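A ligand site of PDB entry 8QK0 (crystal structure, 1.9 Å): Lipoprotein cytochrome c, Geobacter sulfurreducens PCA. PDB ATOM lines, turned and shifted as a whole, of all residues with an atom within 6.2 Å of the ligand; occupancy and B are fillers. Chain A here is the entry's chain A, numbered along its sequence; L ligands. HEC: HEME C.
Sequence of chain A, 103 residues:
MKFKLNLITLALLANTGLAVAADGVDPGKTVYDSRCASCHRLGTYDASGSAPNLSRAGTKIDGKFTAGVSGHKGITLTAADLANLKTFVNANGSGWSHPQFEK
CAB of the ligand is covalently linked to SG of Cys 36 (1.8 Å). CAC of the ligand is covalently linked to SG of Cys 39 (1.8 Å). An iron atom (FE) of the ligand is bound by a ring nitrogen (NE2) of His 40, 1.9 Å away. A ring nitrogen (NE2) of His 72 binds an iron atom (FE) of the ligand (2.3 Å). An oxygen (O1D) of the ligand is in salt-bridge range of the side-chain amino group of Lys 64 (3.4 Å).
O of Cys 39 lies within hydrogen-bond range of N of Ala 51 (3.0 Å). OG of Ser 38 sits at hydrogen-bond distance from SG of Cys 39 (3.7 Å). N of Ser 50 sits at hydrogen-bond distance from O of Cys 39, at 3.1 Å. The backbone carbonyl oxygen (O) of Pro 52 is in hydrogen-bond range of a ring nitrogen (ND1) of His 40 (2.7 Å). The backbone carbonyl oxygen (O) of His 40 lies within hydrogen-bond range of the side-chain hydroxyl (OH) of Tyr 32, at 3.2 Å. NZ of Lys 64 sits at hydrogen-bond distance from ND1 of His 72.
Residues that only touch the ligand: Arg 35 (3.4 Å), Ser 38 (3.6 Å), Ala 51 (3.5 Å), Pro 52 (3.8 Å), Leu 54 (3.99 Å), Lys 60 (3.2 Å), Ile 61 (3.8 Å), Phe 65 (3.4 Å), Lys 73 (3.6 Å), Ile 75 (3.6 Å), Leu 77 (3.9 Å) and Leu 85 (3.7 Å). Hydrophobic or aromatic side chains that line the ligand: His 40, Ala 51, Pro 52, Leu 54, Phe 65, His 72, Ile 75, Leu 77 and Leu 85. Within 4 Å of the ligand: Arg 35, Cys 36, Ser 38, Cys 39, His 40, Ala 51, Pro 52, Leu 54, Lys 60, Ile 61, Lys 64, Phe 65, His 72, Lys 73, Ile 75, Leu 77 and Leu 85.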
ATOM      1  N   VAL A  31      14.652 -25.618  -8.816  1.00  0.00           N
ATOM      2  CA  VAL A  31      15.578 -24.784  -8.068  1.00  0.00           C
ATOM      3  C   VAL A  31      15.010 -24.425  -6.703  1.00  0.00           C
ATOM      4  O   VAL A  31      15.676 -24.594  -5.671  1.00  0.00           O
ATOM      5  CB  VAL A  31      15.936 -23.515  -8.864  1.00  0.00           C
ATOM      6  CG1 VAL A  31      16.658 -22.555  -7.945  1.00  0.00           C
ATOM      7  CG2 VAL A  31      16.798 -23.862 -10.083  1.00  0.00           C
ATOM      8  N   TYR A  32      13.794 -23.881  -6.679  1.00  0.00           N
ATOM      9  CA  TYR A  32      13.205 -23.466  -5.415  1.00  0.00           C
ATOM     10  C   TYR A  32      13.048 -24.662  -4.476  1.00  0.00           C
ATOM     11  O   TYR A  32      13.406 -24.606  -3.295  1.00  0.00           O
ATOM     12  CB  TYR A  32      11.825 -22.837  -5.618  1.00  0.00           C
ATOM     13  CG  TYR A  32      11.235 -22.456  -4.286  1.00  0.00           C
ATOM     14  CD1 TYR A  32      11.705 -21.347  -3.581  1.00  0.00           C
ATOM     15  CD2 TYR A  32      10.333 -23.301  -3.653  1.00  0.00           C
ATOM     16  CE1 TYR A  32      11.208 -21.044  -2.310  1.00  0.00           C
ATOM     17  CE2 TYR A  32       9.851 -23.006  -2.378  1.00  0.00           C
ATOM     18  CZ  TYR A  32      10.298 -21.892  -1.710  1.00  0.00           C
ATOM     19  OH  TYR A  32       9.797 -21.615  -0.453  1.00  0.00           O
ATOM     20  N   ARG A  35      16.506 -26.283  -3.317  1.00  0.00           N
ATOM     21  CA  ARG A  35      17.587 -25.406  -2.858  1.00  0.00           C
ATOM     22  C   ARG A  35      17.196 -24.305  -1.880  1.00  0.00           C
ATOM     23  O   ARG A  35      18.070 -23.870  -1.110  1.00  0.00           O
ATOM     24  CB  ARG A  35      18.310 -24.798  -4.063  1.00  0.00           C
ATOM     25  CG  ARG A  35      18.693 -25.904  -5.044  1.00  0.00           C
ATOM     26  CD  ARG A  35      19.967 -25.603  -5.748  1.00  0.00           C
ATOM     27  NE  ARG A  35      21.121 -25.784  -4.867  1.00  0.00           N
ATOM     28  CZ  ARG A  35      22.350 -25.420  -5.193  1.00  0.00           C
ATOM     29  NH1 ARG A  35      22.618 -24.836  -6.358  1.00  0.00           N
ATOM     30  NH2 ARG A  35      23.342 -25.632  -4.320  1.00  0.00           N
ATOM     31  N   CYS A  36      15.947 -23.884  -1.824  1.00  0.00           N
ATOM     32  CA  CYS A  36      15.549 -22.809  -0.908  1.00  0.00           C
ATOM     33  C   CYS A  36      14.415 -23.191   0.017  1.00  0.00           C
ATOM     34  O   CYS A  36      14.313 -22.604   1.099  1.00  0.00           O
ATOM     35  CB  CYS A  36      15.145 -21.529  -1.676  1.00  0.00           C
ATOM     36  SG  CYS A  36      15.922 -21.237  -3.278  1.00  0.00           S
ATOM     37  N   ALA A  37      13.563 -24.138  -0.380  1.00  0.00           N
ATOM     38  CA  ALA A  37      12.345 -24.426   0.375  1.00  0.00           C
ATOM     39  C   ALA A  37      12.637 -24.968   1.767  1.00  0.00           C
ATOM     40  O   ALA A  37      11.833 -24.751   2.682  1.00  0.00           O
ATOM     41  CB  ALA A  37      11.490 -25.430  -0.384  1.00  0.00           C
ATOM     42  N   SER A  38      13.763 -25.679   1.952  1.00  0.00           N
ATOM     43  CA  SER A  38      14.070 -26.220   3.281  1.00  0.00           C
ATOM     44  C   SER A  38      14.061 -25.130   4.346  1.00  0.00           C
ATOM     45  O   SER A  38      13.798 -25.414   5.522  1.00  0.00           O
ATOM     46  CB  SER A  38      15.433 -26.926   3.258  1.00  0.00           C
ATOM     47  OG  SER A  38      16.482 -26.003   3.077  1.00  0.00           O
ATOM     48  N   CYS A  39      14.320 -23.876   3.954  1.00  0.00           N
ATOM     49  CA  CYS A  39      14.338 -22.744   4.878  1.00  0.00           C
ATOM     50  C   CYS A  39      13.289 -21.681   4.563  1.00  0.00           C
ATOM     51  O   CYS A  39      12.641 -21.170   5.485  1.00  0.00           O
ATOM     52  CB  CYS A  39      15.719 -22.080   4.892  1.00  0.00           C
ATOM     53  SG  CYS A  39      17.074 -23.196   5.352  1.00  0.00           S
ATOM     54  N   HIS A  40      13.112 -21.345   3.297  1.00  0.00           N
ATOM     55  CA  HIS A  40      12.287 -20.208   2.936  1.00  0.00           C
ATOM     56  C   HIS A  40      10.827 -20.605   2.752  1.00  0.00           C
ATOM     57  O   HIS A  40      10.467 -21.791   2.714  1.00  0.00           O
ATOM     58  CB  HIS A  40      12.817 -19.550   1.668  1.00  0.00           C
ATOM     59  CG  HIS A  40      14.031 -18.700   1.886  1.00  0.00           C
ATOM     60  ND1 HIS A  40      13.943 -17.414   2.372  1.00  0.00           N
ATOM     61  CD2 HIS A  40      15.342 -18.930   1.654  1.00  0.00           C
ATOM     62  CE1 HIS A  40      15.148 -16.896   2.465  1.00  0.00           C
ATOM     63  NE2 HIS A  40      16.019 -17.788   2.018  1.00  0.00           N
ATOM     64  N   SER A  50      11.529 -20.941   8.336  1.00  0.00           N
ATOM     65  CA  SER A  50      11.774 -19.822   9.234  1.00  0.00           C
ATOM     66  C   SER A  50      12.360 -18.599   8.527  1.00  0.00           C
ATOM     67  O   SER A  50      12.313 -17.502   9.095  1.00  0.00           O
ATOM     68  CB  SER A  50      12.707 -20.282  10.371  1.00  0.00           C
ATOM     69  OG  SER A  50      13.445 -19.200  10.917  1.00  0.00           O
ATOM     70  N   ALA A  51      12.889 -18.758   7.311  1.00  0.00           N
ATOM     71  CA  ALA A  51      13.500 -17.666   6.571  1.00  0.00           C
ATOM     72  C   ALA A  51      12.421 -16.883   5.809  1.00  0.00           C
ATOM     73  O   ALA A  51      11.290 -17.327   5.680  1.00  0.00           O
ATOM     74  CB  ALA A  51      14.549 -18.231   5.605  1.00  0.00           C
ATOM     75  N   PRO A  52      12.750 -15.677   5.317  1.00  0.00           N
ATOM     76  CA  PRO A  52      11.723 -14.821   4.708  1.00  0.00           C
ATOM     77  C   PRO A  52      10.948 -15.482   3.576  1.00  0.00           C
ATOM     78  O   PRO A  52      11.469 -16.300   2.814  1.00  0.00           O
ATOM     79  CB  PRO A  52      12.521 -13.617   4.206  1.00  0.00           C
ATOM     80  CG  PRO A  52      13.645 -13.517   5.173  1.00  0.00           C
ATOM     81  CD  PRO A  52      14.006 -14.932   5.542  1.00  0.00           C
ATOM     82  N   ASN A  53       9.683 -15.074   3.464  1.00  0.00           N
ATOM     83  CA  ASN A  53       8.903 -15.391   2.286  1.00  0.00           C
ATOM     84  C   ASN A  53       9.526 -14.701   1.072  1.00  0.00           C
ATOM     85  O   ASN A  53       9.756 -13.496   1.078  1.00  0.00           O
ATOM     86  CB  ASN A  53       7.455 -14.945   2.485  1.00  0.00           C
ATOM     87  CG  ASN A  53       6.499 -15.695   1.593  1.00  0.00           C
ATOM     88  OD1 ASN A  53       6.665 -15.706   0.385  1.00  0.00           O
ATOM     89  ND2 ASN A  53       5.516 -16.359   2.190  1.00  0.00           N
ATOM     90  N   LEU A  54       9.827 -15.495   0.036  1.00  0.00           N
ATOM     91  CA  LEU A  54      10.462 -14.952  -1.166  1.00  0.00           C
ATOM     92  C   LEU A  54       9.452 -14.415  -2.199  1.00  0.00           C
ATOM     93  O   LEU A  54       9.847 -14.141  -3.333  1.00  0.00           O
ATOM     94  CB  LEU A  54      11.357 -16.003  -1.805  1.00  0.00           C
ATOM     95  CG  LEU A  54      12.606 -16.300  -0.969  1.00  0.00           C
ATOM     96  CD1 LEU A  54      13.413 -17.450  -1.536  1.00  0.00           C
ATOM     97  CD2 LEU A  54      13.496 -15.068  -0.865  1.00  0.00           C
ATOM     98  N   ALA A  57      10.519 -11.294  -4.321  1.00  0.00           N
ATOM     99  CA  ALA A  57      11.920 -11.102  -3.949  1.00  0.00           C
ATOM    100  C   ALA A  57      12.887 -11.200  -5.127  1.00  0.00           C
ATOM    101  O   ALA A  57      14.087 -11.364  -4.918  1.00  0.00           O
ATOM    102  CB  ALA A  57      12.308 -12.093  -2.838  1.00  0.00           C
ATOM    103  N   LYS A  60      15.737  -8.810  -4.660  1.00  0.00           N
ATOM    104  CA  LYS A  60      16.578  -9.256  -3.550  1.00  0.00           C
ATOM    105  C   LYS A  60      17.355 -10.523  -3.909  1.00  0.00           C
ATOM    106  O   LYS A  60      18.492 -10.695  -3.464  1.00  0.00           O
ATOM    107  CB  LYS A  60      15.726  -9.476  -2.301  1.00  0.00           C
ATOM    108  CG  LYS A  60      15.662  -8.259  -1.403  1.00  0.00           C
ATOM    109  CD  LYS A  60      14.558  -8.418  -0.377  1.00  0.00           C
ATOM    110  CE  LYS A  60      13.850  -7.111  -0.109  1.00  0.00           C
ATOM    111  NZ  LYS A  60      12.354  -7.282  -0.129  1.00  0.00           N
ATOM    112  N   ILE A  61      16.746 -11.425  -4.686  1.00  0.00           N
ATOM    113  CA  ILE A  61      17.450 -12.627  -5.124  1.00  0.00           C
ATOM    114  C   ILE A  61      18.665 -12.258  -5.970  1.00  0.00           C
ATOM    115  O   ILE A  61      19.764 -12.767  -5.775  1.00  0.00           O
ATOM    116  CB  ILE A  61      16.496 -13.564  -5.879  1.00  0.00           C
ATOM    117  CG1 ILE A  61      15.511 -14.221  -4.901  1.00  0.00           C
ATOM    118  CG2 ILE A  61      17.287 -14.670  -6.626  1.00  0.00           C
ATOM    119  CD1 ILE A  61      14.351 -14.974  -5.605  1.00  0.00           C
ATOM    120  N   ASP A  62      18.475 -11.332  -6.930  1.00  0.00           N
ATOM    121  CA  ASP A  62      19.563 -10.951  -7.832  1.00  0.00           C
ATOM    122  C   ASP A  62      20.649 -10.142  -7.111  1.00  0.00           C
ATOM    123  O   ASP A  62      21.809 -10.136  -7.534  1.00  0.00           O
ATOM    124  CB  ASP A  62      19.001 -10.174  -9.037  1.00  0.00           C
ATOM    125  CG  ASP A  62      18.388 -11.088 -10.092  1.00  0.00           C
ATOM    126  OD1 ASP A  62      18.673 -12.303 -10.065  1.00  0.00           O
ATOM    127  OD2 ASP A  62      17.636 -10.591 -10.971  1.00  0.00           O
ATOM    128  N   LYS A  64      21.297 -10.920  -3.885  1.00  0.00           N
ATOM    129  CA  LYS A  64      21.832 -11.891  -2.934  1.00  0.00           C
ATOM    130  C   LYS A  64      22.757 -12.901  -3.607  1.00  0.00           C
ATOM    131  O   LYS A  64      23.653 -13.459  -2.951  1.00  0.00           O
ATOM    132  CB  LYS A  64      20.682 -12.607  -2.228  1.00  0.00           C
ATOM    133  CG  LYS A  64      21.083 -13.748  -1.265  1.00  0.00           C
ATOM    134  CD  LYS A  64      21.906 -13.239  -0.087  1.00  0.00           C
ATOM    135  CE  LYS A  64      21.058 -12.485   0.940  1.00  0.00           C
ATOM    136  NZ  LYS A  64      21.558 -12.792   2.320  1.00  0.00           N
ATOM    137  N   PHE A  65      22.578 -13.130  -4.900  1.00  0.00           N
ATOM    138  CA  PHE A  65      23.287 -14.168  -5.629  1.00  0.00           C
ATOM    139  C   PHE A  65      23.953 -13.590  -6.859  1.00  0.00           C
ATOM    140  O   PHE A  65      23.340 -12.820  -7.613  1.00  0.00           O
ATOM    141  CB  PHE A  65      22.351 -15.296  -6.084  1.00  0.00           C
ATOM    142  CG  PHE A  65      21.989 -16.252  -4.997  1.00  0.00           C
ATOM    143  CD1 PHE A  65      22.848 -17.275  -4.631  1.00  0.00           C
ATOM    144  CD2 PHE A  65      20.776 -16.148  -4.340  1.00  0.00           C
ATOM    145  CE1 PHE A  65      22.511 -18.158  -3.634  1.00  0.00           C
ATOM    146  CE2 PHE A  65      20.450 -17.042  -3.327  1.00  0.00           C
ATOM    147  CZ  PHE A  65      21.320 -18.026  -2.980  1.00  0.00           C
ATOM    148  N   HIS A  72      25.423 -17.498  -0.486  1.00  0.00           N
ATOM    149  CA  HIS A  72      24.385 -17.661   0.508  1.00  0.00           C
ATOM    150  C   HIS A  72      24.111 -19.131   0.835  1.00  0.00           C
ATOM    151  O   HIS A  72      23.738 -19.910  -0.043  1.00  0.00           O
ATOM    152  CB  HIS A  72      23.125 -16.990  -0.042  1.00  0.00           C
ATOM    153  CG  HIS A  72      21.986 -16.941   0.924  1.00  0.00           C
ATOM    154  ND1 HIS A  72      22.031 -16.194   2.089  1.00  0.00           N
ATOM    155  CD2 HIS A  72      20.749 -17.486   0.884  1.00  0.00           C
ATOM    156  CE1 HIS A  72      20.880 -16.306   2.729  1.00  0.00           C
ATOM    157  NE2 HIS A  72      20.103 -17.092   2.025  1.00  0.00           N
ATOM    158  N   LYS A  73      24.325 -19.496   2.108  1.00  0.00           N
ATOM    159  CA  LYS A  73      24.067 -20.849   2.616  1.00  0.00           C
ATOM    160  C   LYS A  73      24.798 -21.921   1.797  1.00  0.00           C
ATOM    161  O   LYS A  73      24.296 -23.028   1.628  1.00  0.00           O
ATOM    162  CB  LYS A  73      22.568 -21.168   2.671  1.00  0.00           C
ATOM    163  CG  LYS A  73      21.727 -20.196   3.502  1.00  0.00           C
ATOM    164  CD  LYS A  73      22.385 -19.933   4.855  1.00  0.00           C
ATOM    165  CE  LYS A  73      21.699 -18.827   5.614  1.00  0.00           C
ATOM    166  NZ  LYS A  73      21.725 -19.064   7.071  1.00  0.00           N
ATOM    167  N   ILE A  75      25.160 -22.086  -1.307  1.00  0.00           N
ATOM    168  CA  ILE A  75      24.524 -22.305  -2.599  1.00  0.00           C
ATOM    169  C   ILE A  75      25.319 -21.604  -3.693  1.00  0.00           C
ATOM    170  O   ILE A  75      25.789 -20.474  -3.507  1.00  0.00           O
ATOM    171  CB  ILE A  75      23.080 -21.805  -2.554  1.00  0.00           C
ATOM    172  CG1 ILE A  75      22.250 -22.628  -1.536  1.00  0.00           C
ATOM    173  CG2 ILE A  75      22.433 -21.819  -3.959  1.00  0.00           C
ATOM    174  CD1 ILE A  75      21.080 -21.847  -0.915  1.00  0.00           C
ATOM    175  N   LEU A  77      24.472 -20.728  -7.823  1.00  0.00           N
ATOM    176  CA  LEU A  77      23.408 -20.729  -8.826  1.00  0.00           C
ATOM    177  C   LEU A  77      23.993 -20.315 -10.170  1.00  0.00           C
ATOM    178  O   LEU A  77      24.756 -19.340 -10.238  1.00  0.00           O
ATOM    179  CB  LEU A  77      22.265 -19.783  -8.436  1.00  0.00           C
ATOM    180  CG  LEU A  77      21.486 -20.037  -7.146  1.00  0.00           C
ATOM    181  CD1 LEU A  77      20.262 -19.128  -7.049  1.00  0.00           C
ATOM    182  CD2 LEU A  77      21.083 -21.508  -7.045  1.00  0.00           C
ATOM    183  N   LEU A  85      14.445 -19.576 -11.560  1.00  0.00           N
ATOM    184  CA  LEU A  85      13.861 -19.458 -10.227  1.00  0.00           C
ATOM    185  C   LEU A  85      12.981 -18.210 -10.105  1.00  0.00           C
ATOM    186  O   LEU A  85      11.869 -18.272  -9.586  1.00  0.00           O
ATOM    187  CB  LEU A  85      14.975 -19.440  -9.166  1.00  0.00           C
ATOM    188  CG  LEU A  85      14.641 -18.897  -7.783  1.00  0.00           C
ATOM    189  CD1 LEU A  85      13.727 -19.879  -7.122  1.00  0.00           C
ATOM    190  CD2 LEU A  85      15.931 -18.737  -6.931  1.00  0.00           C
HETATM  191 FE   HEC L   1      17.867 -17.521   2.008  1.00  0.00          FE
HETATM  192  CHA HEC L   1      17.599 -14.416   3.531  1.00  0.00           C
HETATM  193  CHB HEC L   1      17.430 -16.028  -1.022  1.00  0.00           C
HETATM  194  CHC HEC L   1      18.023 -20.630   0.439  1.00  0.00           C
HETATM  195  CHD HEC L   1      18.088 -19.084   5.058  1.00  0.00           C
HETATM  196  NA  HEC L   1      17.594 -15.568   1.369  1.00  0.00           N
HETATM  197  C1A HEC L   1      17.467 -14.440   2.160  1.00  0.00           C
HETATM  198  C2A HEC L   1      17.200 -13.300   1.280  1.00  0.00           C
HETATM  199  C3A HEC L   1      17.159 -13.752   0.026  1.00  0.00           C
HETATM  200  C4A HEC L   1      17.395 -15.179   0.061  1.00  0.00           C
HETATM  201  CMA HEC L   1      16.873 -12.879  -1.228  1.00  0.00           C
HETATM  202  CAA HEC L   1      16.981 -11.834   1.706  1.00  0.00           C
HETATM  203  CBA HEC L   1      15.681 -11.797   2.502  1.00  0.00           C
HETATM  204  CGA HEC L   1      15.124 -10.394   2.559  1.00  0.00           C
HETATM  205  O1A HEC L   1      15.911  -9.443   2.304  1.00  0.00           O
HETATM  206  O2A HEC L   1      13.904 -10.244   2.850  1.00  0.00           O
HETATM  207  NB  HEC L   1      17.795 -18.233   0.097  1.00  0.00           N
HETATM  208  C1B HEC L   1      17.543 -17.401  -0.994  1.00  0.00           C
HETATM  209  C2B HEC L   1      17.443 -18.218  -2.168  1.00  0.00           C
HETATM  210  C3B HEC L   1      17.586 -19.502  -1.823  1.00  0.00           C
HETATM  211  C4B HEC L   1      17.816 -19.531  -0.361  1.00  0.00           C
HETATM  212  CMB HEC L   1      17.152 -17.650  -3.592  1.00  0.00           C
HETATM  213  CAB HEC L   1      17.531 -20.701  -2.803  1.00  0.00           C
HETATM  214  CBB HEC L   1      18.649 -20.670  -3.873  1.00  0.00           C
HETATM  215  NC  HEC L   1      18.003 -19.525   2.659  1.00  0.00           N
HETATM  216  C1C HEC L   1      18.123 -20.632   1.832  1.00  0.00           C
HETATM  217  C2C HEC L   1      18.484 -21.760   2.678  1.00  0.00           C
HETATM  218  C3C HEC L   1      18.372 -21.352   3.971  1.00  0.00           C
HETATM  219  C4C HEC L   1      18.148 -19.919   3.956  1.00  0.00           C
HETATM  220  CMC HEC L   1      18.545 -23.221   2.161  1.00  0.00           C
HETATM  221  CAC HEC L   1      18.549 -22.228   5.255  1.00  0.00           C
HETATM  222  CBC HEC L   1      19.845 -23.053   5.306  1.00  0.00           C
HETATM  223  ND  HEC L   1      17.822 -16.850   3.955  1.00  0.00           N
HETATM  224  C1D HEC L   1      17.988 -17.712   5.056  1.00  0.00           C
HETATM  225  C2D HEC L   1      18.006 -16.925   6.258  1.00  0.00           C
HETATM  226  C3D HEC L   1      17.858 -15.464   5.795  1.00  0.00           C
HETATM  227  C4D HEC L   1      17.760 -15.516   4.354  1.00  0.00           C
HETATM  228  CMD HEC L   1      18.161 -17.422   7.712  1.00  0.00           C
HETATM  229  CAD HEC L   1      17.824 -14.215   6.695  1.00  0.00           C
HETATM  230  CBD HEC L   1      19.286 -13.876   7.027  1.00  0.00           C
HETATM  231  CGD HEC L   1      19.968 -13.434   5.758  1.00  0.00           C
HETATM  232  O1D HEC L   1      21.062 -13.966   5.445  1.00  0.00           O
HETATM  233  O2D HEC L   1      19.408 -12.539   5.064  1.00  0.00           O
